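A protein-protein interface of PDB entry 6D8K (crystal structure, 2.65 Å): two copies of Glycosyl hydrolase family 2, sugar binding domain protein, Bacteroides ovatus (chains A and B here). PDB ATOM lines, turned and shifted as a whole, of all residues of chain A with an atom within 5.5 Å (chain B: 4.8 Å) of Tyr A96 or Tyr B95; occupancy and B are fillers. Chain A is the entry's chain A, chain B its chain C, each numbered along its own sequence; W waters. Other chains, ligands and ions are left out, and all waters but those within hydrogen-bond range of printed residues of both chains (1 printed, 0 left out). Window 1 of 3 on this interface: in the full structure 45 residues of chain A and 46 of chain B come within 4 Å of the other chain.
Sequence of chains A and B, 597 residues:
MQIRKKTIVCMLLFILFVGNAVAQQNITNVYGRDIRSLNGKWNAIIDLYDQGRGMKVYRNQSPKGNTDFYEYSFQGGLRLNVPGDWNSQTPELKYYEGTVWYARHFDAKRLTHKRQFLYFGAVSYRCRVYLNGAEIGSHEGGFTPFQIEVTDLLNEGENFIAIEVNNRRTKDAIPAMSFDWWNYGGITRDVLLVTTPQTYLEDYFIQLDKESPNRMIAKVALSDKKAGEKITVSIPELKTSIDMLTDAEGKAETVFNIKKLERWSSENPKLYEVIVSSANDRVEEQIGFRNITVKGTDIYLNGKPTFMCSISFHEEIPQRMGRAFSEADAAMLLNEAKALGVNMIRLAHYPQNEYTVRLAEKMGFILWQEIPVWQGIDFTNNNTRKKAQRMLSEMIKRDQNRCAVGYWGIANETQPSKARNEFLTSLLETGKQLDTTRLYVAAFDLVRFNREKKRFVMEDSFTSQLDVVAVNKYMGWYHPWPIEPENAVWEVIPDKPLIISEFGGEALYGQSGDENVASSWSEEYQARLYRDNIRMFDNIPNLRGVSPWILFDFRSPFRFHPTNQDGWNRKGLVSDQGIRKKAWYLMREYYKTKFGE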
ATOM      1  N   ILE A  46      10.356  13.101  11.194  1.00  0.00           N
ATOM      2  CA  ILE A  46      10.538  14.551  11.112  1.00  0.00           C
ATOM      3  C   ILE A  46       9.394  15.135  10.304  1.00  0.00           C
ATOM      4  O   ILE A  46       9.196  14.740   9.149  1.00  0.00           O
ATOM      5  CB  ILE A  46      11.893  14.881  10.465  1.00  0.00           C
ATOM      6  CG1 ILE A  46      12.977  14.091  11.184  1.00  0.00           C
ATOM      7  CG2 ILE A  46      12.186  16.355  10.541  1.00  0.00           C
ATOM      8  CD1 ILE A  46      14.265  13.982  10.419  1.00  0.00           C
ATOM      9  N   ASP A  47       8.661  16.098  10.883  1.00  0.00           N
ATOM     10  CA  ASP A  47       7.430  16.646  10.287  1.00  0.00           C
ATOM     11  C   ASP A  47       7.554  18.160  10.085  1.00  0.00           C
ATOM     12  O   ASP A  47       6.856  18.926  10.759  1.00  0.00           O
ATOM     13  CB  ASP A  47       6.156  16.285  11.210  1.00  0.00           C
ATOM     14  CG  ASP A  47       4.800  16.746  10.598  1.00  0.00           C
ATOM     15  OD1 ASP A  47       4.763  17.265   9.453  1.00  0.00           O
ATOM     16  OD2 ASP A  47       3.761  16.579  11.271  1.00  0.00           O
ATOM     17  N   LEU A  48       8.383  18.586   9.117  1.00  0.00           N
ATOM     18  CA  LEU A  48       8.728  20.004   8.992  1.00  0.00           C
ATOM     19  C   LEU A  48       7.499  20.898   8.830  1.00  0.00           C
ATOM     20  O   LEU A  48       7.399  21.942   9.485  1.00  0.00           O
ATOM     21  CB  LEU A  48       9.693  20.236   7.827  1.00  0.00           C
ATOM     22  CG  LEU A  48      10.131  21.710   7.723  1.00  0.00           C
ATOM     23  CD1 LEU A  48      10.844  22.153   8.988  1.00  0.00           C
ATOM     24  CD2 LEU A  48      11.028  21.977   6.507  1.00  0.00           C
ATOM     25  N   TRP A  86      17.052  15.583  20.283  1.00  0.00           N
ATOM     26  CA  TRP A  86      17.225  15.051  18.943  1.00  0.00           C
ATOM     27  C   TRP A  86      18.369  15.719  18.203  1.00  0.00           C
ATOM     28  O   TRP A  86      18.919  15.109  17.287  1.00  0.00           O
ATOM     29  CB  TRP A  86      15.925  15.143  18.125  1.00  0.00           C
ATOM     30  CG  TRP A  86      15.388  16.532  17.821  1.00  0.00           C
ATOM     31  CD1 TRP A  86      16.037  17.543  17.206  1.00  0.00           C
ATOM     32  CD2 TRP A  86      14.069  17.009  18.089  1.00  0.00           C
ATOM     33  NE1 TRP A  86      15.222  18.632  17.085  1.00  0.00           N
ATOM     34  CE2 TRP A  86      14.006  18.331  17.628  1.00  0.00           C
ATOM     35  CE3 TRP A  86      12.942  16.449  18.695  1.00  0.00           C
ATOM     36  CZ2 TRP A  86      12.859  19.105  17.746  1.00  0.00           C
ATOM     37  CZ3 TRP A  86      11.813  17.203  18.805  1.00  0.00           C
ATOM     38  CH2 TRP A  86      11.772  18.521  18.326  1.00  0.00           C
ATOM     39  N   ASN A  87      18.791  16.899  18.658  1.00  0.00           N
ATOM     40  CA  ASN A  87      19.688  17.765  17.890  1.00  0.00           C
ATOM     41  C   ASN A  87      21.054  17.126  17.641  1.00  0.00           C
ATOM     42  O   ASN A  87      21.662  17.334  16.583  1.00  0.00           O
ATOM     43  CB  ASN A  87      19.840  19.104  18.623  1.00  0.00           C
ATOM     44  CG  ASN A  87      18.516  19.861  18.721  1.00  0.00           C
ATOM     45  OD1 ASN A  87      17.670  19.580  19.596  1.00  0.00           O
ATOM     46  ND2 ASN A  87      18.304  20.779  17.787  1.00  0.00           N
ATOM     47  N   GLU A  92      21.349  16.403  10.364  1.00  0.00           N
ATOM     48  CA  GLU A  92      20.160  17.051   9.829  1.00  0.00           C
ATOM     49  C   GLU A  92      19.263  17.635  10.915  1.00  0.00           C
ATOM     50  O   GLU A  92      18.460  18.519  10.614  1.00  0.00           O
ATOM     51  CB  GLU A  92      19.361  16.044   8.987  1.00  0.00           C
ATOM     52  CG  GLU A  92      20.020  15.626   7.656  1.00  0.00           C
ATOM     53  CD  GLU A  92      19.468  14.317   7.052  1.00  0.00           C
ATOM     54  OE1 GLU A  92      20.302  13.523   6.564  1.00  0.00           O
ATOM     55  OE2 GLU A  92      18.227  14.071   7.044  1.00  0.00           O
ATOM     56  N   LEU A  93      19.369  17.161  12.161  1.00  0.00           N
ATOM     57  CA  LEU A  93      18.495  17.618  13.239  1.00  0.00           C
ATOM     58  C   LEU A  93      19.148  18.647  14.137  1.00  0.00           C
ATOM     59  O   LEU A  93      18.469  19.209  15.006  1.00  0.00           O
ATOM     60  CB  LEU A  93      18.016  16.434  14.089  1.00  0.00           C
ATOM     61  CG  LEU A  93      16.972  15.539  13.416  1.00  0.00           C
ATOM     62  CD1 LEU A  93      16.503  14.462  14.409  1.00  0.00           C
ATOM     63  CD2 LEU A  93      15.800  16.353  12.871  1.00  0.00           C
ATOM     64  N   LYS A  94      20.436  18.911  13.938  1.00  0.00           N
ATOM     65  CA  LYS A  94      21.153  19.845  14.791  1.00  0.00           C
ATOM     66  C   LYS A  94      20.416  21.176  14.929  1.00  0.00           C
ATOM     67  O   LYS A  94      20.246  21.684  16.035  1.00  0.00           O
ATOM     68  CB  LYS A  94      22.574  20.049  14.252  1.00  0.00           C
ATOM     69  CG  LYS A  94      23.385  20.952  15.102  1.00  0.00           C
ATOM     70  CD  LYS A  94      24.732  21.246  14.519  1.00  0.00           C
ATOM     71  CE  LYS A  94      25.477  22.229  15.454  1.00  0.00           C
ATOM     72  NZ  LYS A  94      26.796  22.621  14.936  1.00  0.00           N
ATOM     73  N   TYR A  95      19.986  21.774  13.820  1.00  0.00           N
ATOM     74  CA  TYR A  95      19.241  23.029  13.908  1.00  0.00           C
ATOM     75  C   TYR A  95      17.753  22.840  13.739  1.00  0.00           C
ATOM     76  O   TYR A  95      17.053  23.822  13.508  1.00  0.00           O
ATOM     77  CB  TYR A  95      19.681  24.030  12.857  1.00  0.00           C
ATOM     78  CG  TYR A  95      21.060  24.563  12.994  1.00  0.00           C
ATOM     79  CD1 TYR A  95      22.132  23.833  12.521  1.00  0.00           C
ATOM     80  CD2 TYR A  95      21.300  25.820  13.534  1.00  0.00           C
ATOM     81  CE1 TYR A  95      23.394  24.304  12.596  1.00  0.00           C
ATOM     82  CE2 TYR A  95      22.592  26.298  13.638  1.00  0.00           C
ATOM     83  CZ  TYR A  95      23.634  25.525  13.154  1.00  0.00           C
ATOM     84  OH  TYR A  95      24.931  25.954  13.225  1.00  0.00           O
ATOM     85  N   TYR A  96      17.251  21.621  13.845  1.00  0.00           N
ATOM     86  CA  TYR A  96      15.851  21.394  13.544  1.00  0.00           C
ATOM     87  C   TYR A  96      14.942  22.047  14.575  1.00  0.00           C
ATOM     88  O   TYR A  96      14.980  21.705  15.763  1.00  0.00           O
ATOM     89  CB  TYR A  96      15.547  19.897  13.462  1.00  0.00           C
ATOM     90  CG  TYR A  96      14.108  19.688  13.075  1.00  0.00           C
ATOM     91  CD1 TYR A  96      13.685  19.898  11.763  1.00  0.00           C
ATOM     92  CD2 TYR A  96      13.171  19.334  14.025  1.00  0.00           C
ATOM     93  CE1 TYR A  96      12.373  19.742  11.402  1.00  0.00           C
ATOM     94  CE2 TYR A  96      11.849  19.176  13.689  1.00  0.00           C
ATOM     95  CZ  TYR A  96      11.447  19.374  12.373  1.00  0.00           C
ATOM     96  OH  TYR A  96      10.126  19.198  12.031  1.00  0.00           O
ATOM     97  N   GLU A  97      14.087  22.940  14.103  1.00  0.00           N
ATOM     98  CA  GLU A  97      12.956  23.434  14.876  1.00  0.00           C
ATOM     99  C   GLU A  97      11.650  23.026  14.216  1.00  0.00           C
ATOM    100  O   GLU A  97      11.491  23.152  12.999  1.00  0.00           O
ATOM    101  CB  GLU A  97      12.985  24.941  15.010  1.00  0.00           C
ATOM    102  CG  GLU A  97      14.281  25.458  15.507  1.00  0.00           C
ATOM    103  CD  GLU A  97      14.159  26.873  16.036  1.00  0.00           C
ATOM    104  OE1 GLU A  97      13.332  27.650  15.486  1.00  0.00           O
ATOM    105  OE2 GLU A  97      14.872  27.182  17.012  1.00  0.00           O
ATOM    106  N   GLY A  98      10.718  22.577  15.028  1.00  0.00           N
ATOM    107  CA  GLY A  98       9.417  22.148  14.588  1.00  0.00           C
ATOM    108  C   GLY A  98       8.961  20.938  15.390  1.00  0.00           C
ATOM    109  O   GLY A  98       9.238  20.833  16.579  1.00  0.00           O
ATOM    110  N   THR A  99       8.232  20.068  14.709  1.00  0.00           N
ATOM    111  CA  THR A  99       7.631  18.872  15.273  1.00  0.00           C
ATOM    112  C   THR A  99       8.447  17.635  14.902  1.00  0.00           C
ATOM    113  O   THR A  99       8.880  17.481  13.748  1.00  0.00           O
ATOM    114  CB  THR A  99       6.197  18.725  14.750  1.00  0.00           C
ATOM    115  OG1 THR A  99       5.370  19.768  15.300  1.00  0.00           O
ATOM    116  CG2 THR A  99       5.625  17.360  15.072  1.00  0.00           C
ATOM    117  N   VAL A 100       8.675  16.758  15.880  1.00  0.00           N
ATOM    118  CA  VAL A 100       9.141  15.399  15.625  1.00  0.00           C
ATOM    119  C   VAL A 100       8.180  14.431  16.318  1.00  0.00           C
ATOM    120  O   VAL A 100       7.786  14.660  17.463  1.00  0.00           O
ATOM    121  CB  VAL A 100      10.590  15.183  16.101  1.00  0.00           C
ATOM    122  CG1 VAL A 100      11.051  13.732  15.869  1.00  0.00           C
ATOM    123  CG2 VAL A 100      11.547  16.187  15.420  1.00  0.00           C
ATOM    124  N   ASN A 167       9.239  22.088  19.196  1.00  0.00           N
ATOM    125  CA  ASN A 167      10.120  23.068  19.833  1.00  0.00           C
ATOM    126  C   ASN A 167      10.164  24.419  19.099  1.00  0.00           C
ATOM    127  O   ASN A 167      11.174  25.139  19.167  1.00  0.00           O
ATOM    128  CB  ASN A 167      11.547  22.505  19.998  1.00  0.00           C
ATOM    129  CG  ASN A 167      12.349  22.479  18.695  1.00  0.00           C
ATOM    130  OD1 ASN A 167      11.801  22.452  17.601  1.00  0.00           O
ATOM    131  ND2 ASN A 167      13.659  22.482  18.823  1.00  0.00           N
ATOM    132  N   ASN A 183      18.350  25.343  21.302  1.00  0.00           N
ATOM    133  CA  ASN A 183      16.943  24.937  21.355  1.00  0.00           C
ATOM    134  C   ASN A 183      16.825  23.432  21.118  1.00  0.00           C
ATOM    135  O   ASN A 183      16.318  22.960  20.101  1.00  0.00           O
ATOM    136  CB  ASN A 183      16.096  25.677  20.342  1.00  0.00           C
ATOM    137  CG  ASN A 183      14.625  25.430  20.567  1.00  0.00           C
ATOM    138  OD1 ASN A 183      14.230  25.036  21.678  1.00  0.00           O
ATOM    139  ND2 ASN A 183      13.795  25.672  19.537  1.00  0.00           N
ATOM    140  N   GLU B  92      23.718  19.742   7.855  1.00  0.00           N
ATOM    141  CA  GLU B  92      23.166  20.554   8.937  1.00  0.00           C
ATOM    142  C   GLU B  92      22.118  21.531   8.426  1.00  0.00           C
ATOM    143  O   GLU B  92      21.231  21.944   9.180  1.00  0.00           O
ATOM    144  CB  GLU B  92      24.274  21.344   9.649  1.00  0.00           C
ATOM    145  CG  GLU B  92      25.255  20.548  10.522  1.00  0.00           C
ATOM    146  CD  GLU B  92      26.395  19.912   9.724  1.00  0.00           C
ATOM    147  OE1 GLU B  92      27.273  19.268  10.339  1.00  0.00           O
ATOM    148  OE2 GLU B  92      26.422  20.050   8.483  1.00  0.00           O
ATOM    149  N   LEU B  93      22.215  21.932   7.159  1.00  0.00           N
ATOM    150  CA  LEU B  93      21.344  22.945   6.580  1.00  0.00           C
ATOM    151  C   LEU B  93      20.101  22.374   5.923  1.00  0.00           C
ATOM    152  O   LEU B  93      19.233  23.145   5.505  1.00  0.00           O
ATOM    153  CB  LEU B  93      22.134  23.758   5.569  1.00  0.00           C
ATOM    154  CG  LEU B  93      22.993  24.777   6.295  1.00  0.00           C
ATOM    155  CD1 LEU B  93      24.185  25.206   5.428  1.00  0.00           C
ATOM    156  CD2 LEU B  93      22.137  25.976   6.684  1.00  0.00           C
ATOM    157  N   LYS B  94      19.984  21.050   5.869  1.00  0.00           N
ATOM    158  CA  LYS B  94      18.933  20.410   5.089  1.00  0.00           C
ATOM    159  C   LYS B  94      17.544  20.878   5.515  1.00  0.00           C
ATOM    160  O   LYS B  94      16.723  21.252   4.669  1.00  0.00           O
ATOM    161  CB  LYS B  94      19.068  18.891   5.208  1.00  0.00           C
ATOM    162  CG  LYS B  94      18.018  18.100   4.474  1.00  0.00           C
ATOM    163  CD  LYS B  94      18.530  16.695   4.197  1.00  0.00           C
ATOM    164  CE  LYS B  94      17.585  15.921   3.298  1.00  0.00           C
ATOM    165  NZ  LYS B  94      18.118  14.565   3.126  1.00  0.00           N
ATOM    166  N   TYR B  95      17.247  20.865   6.819  1.00  0.00           N
ATOM    167  CA  TYR B  95      15.924  21.301   7.252  1.00  0.00           C
ATOM    168  C   TYR B  95      15.928  22.705   7.794  1.00  0.00           C
ATOM    169  O   TYR B  95      14.909  23.139   8.329  1.00  0.00           O
ATOM    170  CB  TYR B  95      15.313  20.378   8.318  1.00  0.00           C
ATOM    171  CG  TYR B  95      15.059  18.966   7.888  1.00  0.00           C
ATOM    172  CD1 TYR B  95      16.120  18.103   7.660  1.00  0.00           C
ATOM    173  CD2 TYR B  95      13.766  18.484   7.714  1.00  0.00           C
ATOM    174  CE1 TYR B  95      15.908  16.797   7.257  1.00  0.00           C
ATOM    175  CE2 TYR B  95      13.540  17.174   7.328  1.00  0.00           C
ATOM    176  CZ  TYR B  95      14.615  16.331   7.097  1.00  0.00           C
ATOM    177  OH  TYR B  95      14.413  15.027   6.717  1.00  0.00           O
ATOM    178  N   TYR B  96      17.040  23.416   7.667  1.00  0.00           N
ATOM    179  CA  TYR B  96      17.150  24.752   8.219  1.00  0.00           C
ATOM    180  C   TYR B  96      16.103  25.680   7.618  1.00  0.00           C
ATOM    181  O   TYR B  96      16.079  25.922   6.404  1.00  0.00           O
ATOM    182  CB  TYR B  96      18.548  25.334   7.998  1.00  0.00           C
ATOM    183  CG  TYR B  96      18.674  26.666   8.719  1.00  0.00           C
ATOM    184  CD1 TYR B  96      19.002  26.724  10.089  1.00  0.00           C
ATOM    185  CD2 TYR B  96      18.374  27.859   8.065  1.00  0.00           C
ATOM    186  CE1 TYR B  96      19.059  27.940  10.755  1.00  0.00           C
ATOM    187  CE2 TYR B  96      18.431  29.077   8.727  1.00  0.00           C
ATOM    188  CZ  TYR B  96      18.778  29.124  10.058  1.00  0.00           C
ATOM    189  OH  TYR B  96      18.837  30.350  10.686  1.00  0.00           O
ATOM    190  N   GLU B  97      15.247  26.213   8.476  1.00  0.00           N
ATOM    191  CA  GLU B  97      14.474  27.396   8.162  1.00  0.00           C
ATOM    192  C   GLU B  97      14.868  28.514   9.110  1.00  0.00           C
ATOM    193  O   GLU B  97      15.170  28.265  10.280  1.00  0.00           O
ATOM    194  CB  GLU B  97      12.980  27.141   8.262  1.00  0.00           C
ATOM    195  CG  GLU B  97      12.490  25.969   7.453  1.00  0.00           C
ATOM    196  CD  GLU B  97      11.029  25.704   7.697  1.00  0.00           C
ATOM    197  OE1 GLU B  97      10.599  25.923   8.853  1.00  0.00           O
ATOM    198  OE2 GLU B  97      10.318  25.306   6.741  1.00  0.00           O
ATOM    199  N   TRP B 182      10.104  21.380  -1.276  1.00  0.00           N
ATOM    200  CA  TRP B 182      11.021  21.706  -0.192  1.00  0.00           C
ATOM    201  C   TRP B 182      11.173  23.211  -0.073  1.00  0.00           C
ATOM    202  O   TRP B 182      11.152  23.942  -1.076  1.00  0.00           O
ATOM    203  CB  TRP B 182      12.389  21.069  -0.418  1.00  0.00           C
ATOM    204  CG  TRP B 182      13.078  20.653   0.824  1.00  0.00           C
ATOM    205  CD1 TRP B 182      14.015  21.351   1.509  1.00  0.00           C
ATOM    206  CD2 TRP B 182      12.908  19.408   1.530  1.00  0.00           C
ATOM    207  NE1 TRP B 182      14.438  20.640   2.600  1.00  0.00           N
ATOM    208  CE2 TRP B 182      13.778  19.442   2.637  1.00  0.00           C
ATOM    209  CE3 TRP B 182      12.101  18.267   1.329  1.00  0.00           C
ATOM    210  CZ2 TRP B 182      13.873  18.393   3.540  1.00  0.00           C
ATOM    211  CZ3 TRP B 182      12.195  17.221   2.226  1.00  0.00           C
ATOM    212  CH2 TRP B 182      13.077  17.292   3.322  1.00  0.00           C
HETATM  213  O   HOH W   1      11.584  25.683  11.590  1.00  0.00           O
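Hydrophobic or aromatic side chains of chain B within 4 Å of the printed part of chain A: Tyr B95 and Tyr B96.
Among the printed residues, merely in contact across the chains: Leu A48 with Glu B97, Ile A46 with Tyr B95, Glu A92 with Tyr B95, Tyr A96 with Tyr B95, Tyr A95 with Tyr B96 and Tyr A95 with Glu B92.
O of Lys B94 lies within hydrogen-bond range of NE1 of Trp B182, at 3.1 Å. The side-chain hydroxyl of Tyr A96 is in hydrogen-bond range of the backbone carbonyl oxygen of Thr A99, at 2.7 Å. The indole nitrogen (NE1) of Trp A86 is in hydrogen-bond range of the backbone carbonyl oxygen (O) of Tyr A96, 3.4 Å away. The side-chain hydroxyl of Tyr A96 lies close to the backbone NH of Leu A48, 3.5 Å away. O of Tyr A96 sits at hydrogen-bond distance from ND2 of Asn A167 (3.4 Å).
Water W1 bridges O of Glu A97 and OE1 of Glu B97.
Of the printed residues of chain B, Glu A92 touches Lys B94 and Tyr B95. Of the printed residues of chain B, Tyr A95 touches Glu B92 (3.9 Å) and Tyr B96 (3.9 Å). Tyr A96 touches just one residue of chain B: Tyr B95. Glu A97 touches none of the printed residues of chain B.
Glu A92 touches Lys B94, but with the chains exchanged Lys A94 does not touch Glu B92 (4.1 Å). Glu A92 touches Tyr B95, and with the chains exchanged Tyr A95 touches Glu B92. Tyr A95 touches Tyr B96, and with the chains exchanged Tyr A96 touches Tyr B95. Positions printed for both chains: 92, 93, 94, 95, 96 and 97.
OE2 of Glu A92 lies within salt-bridge range of NZ of Lys B94, 3.95 Å away.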
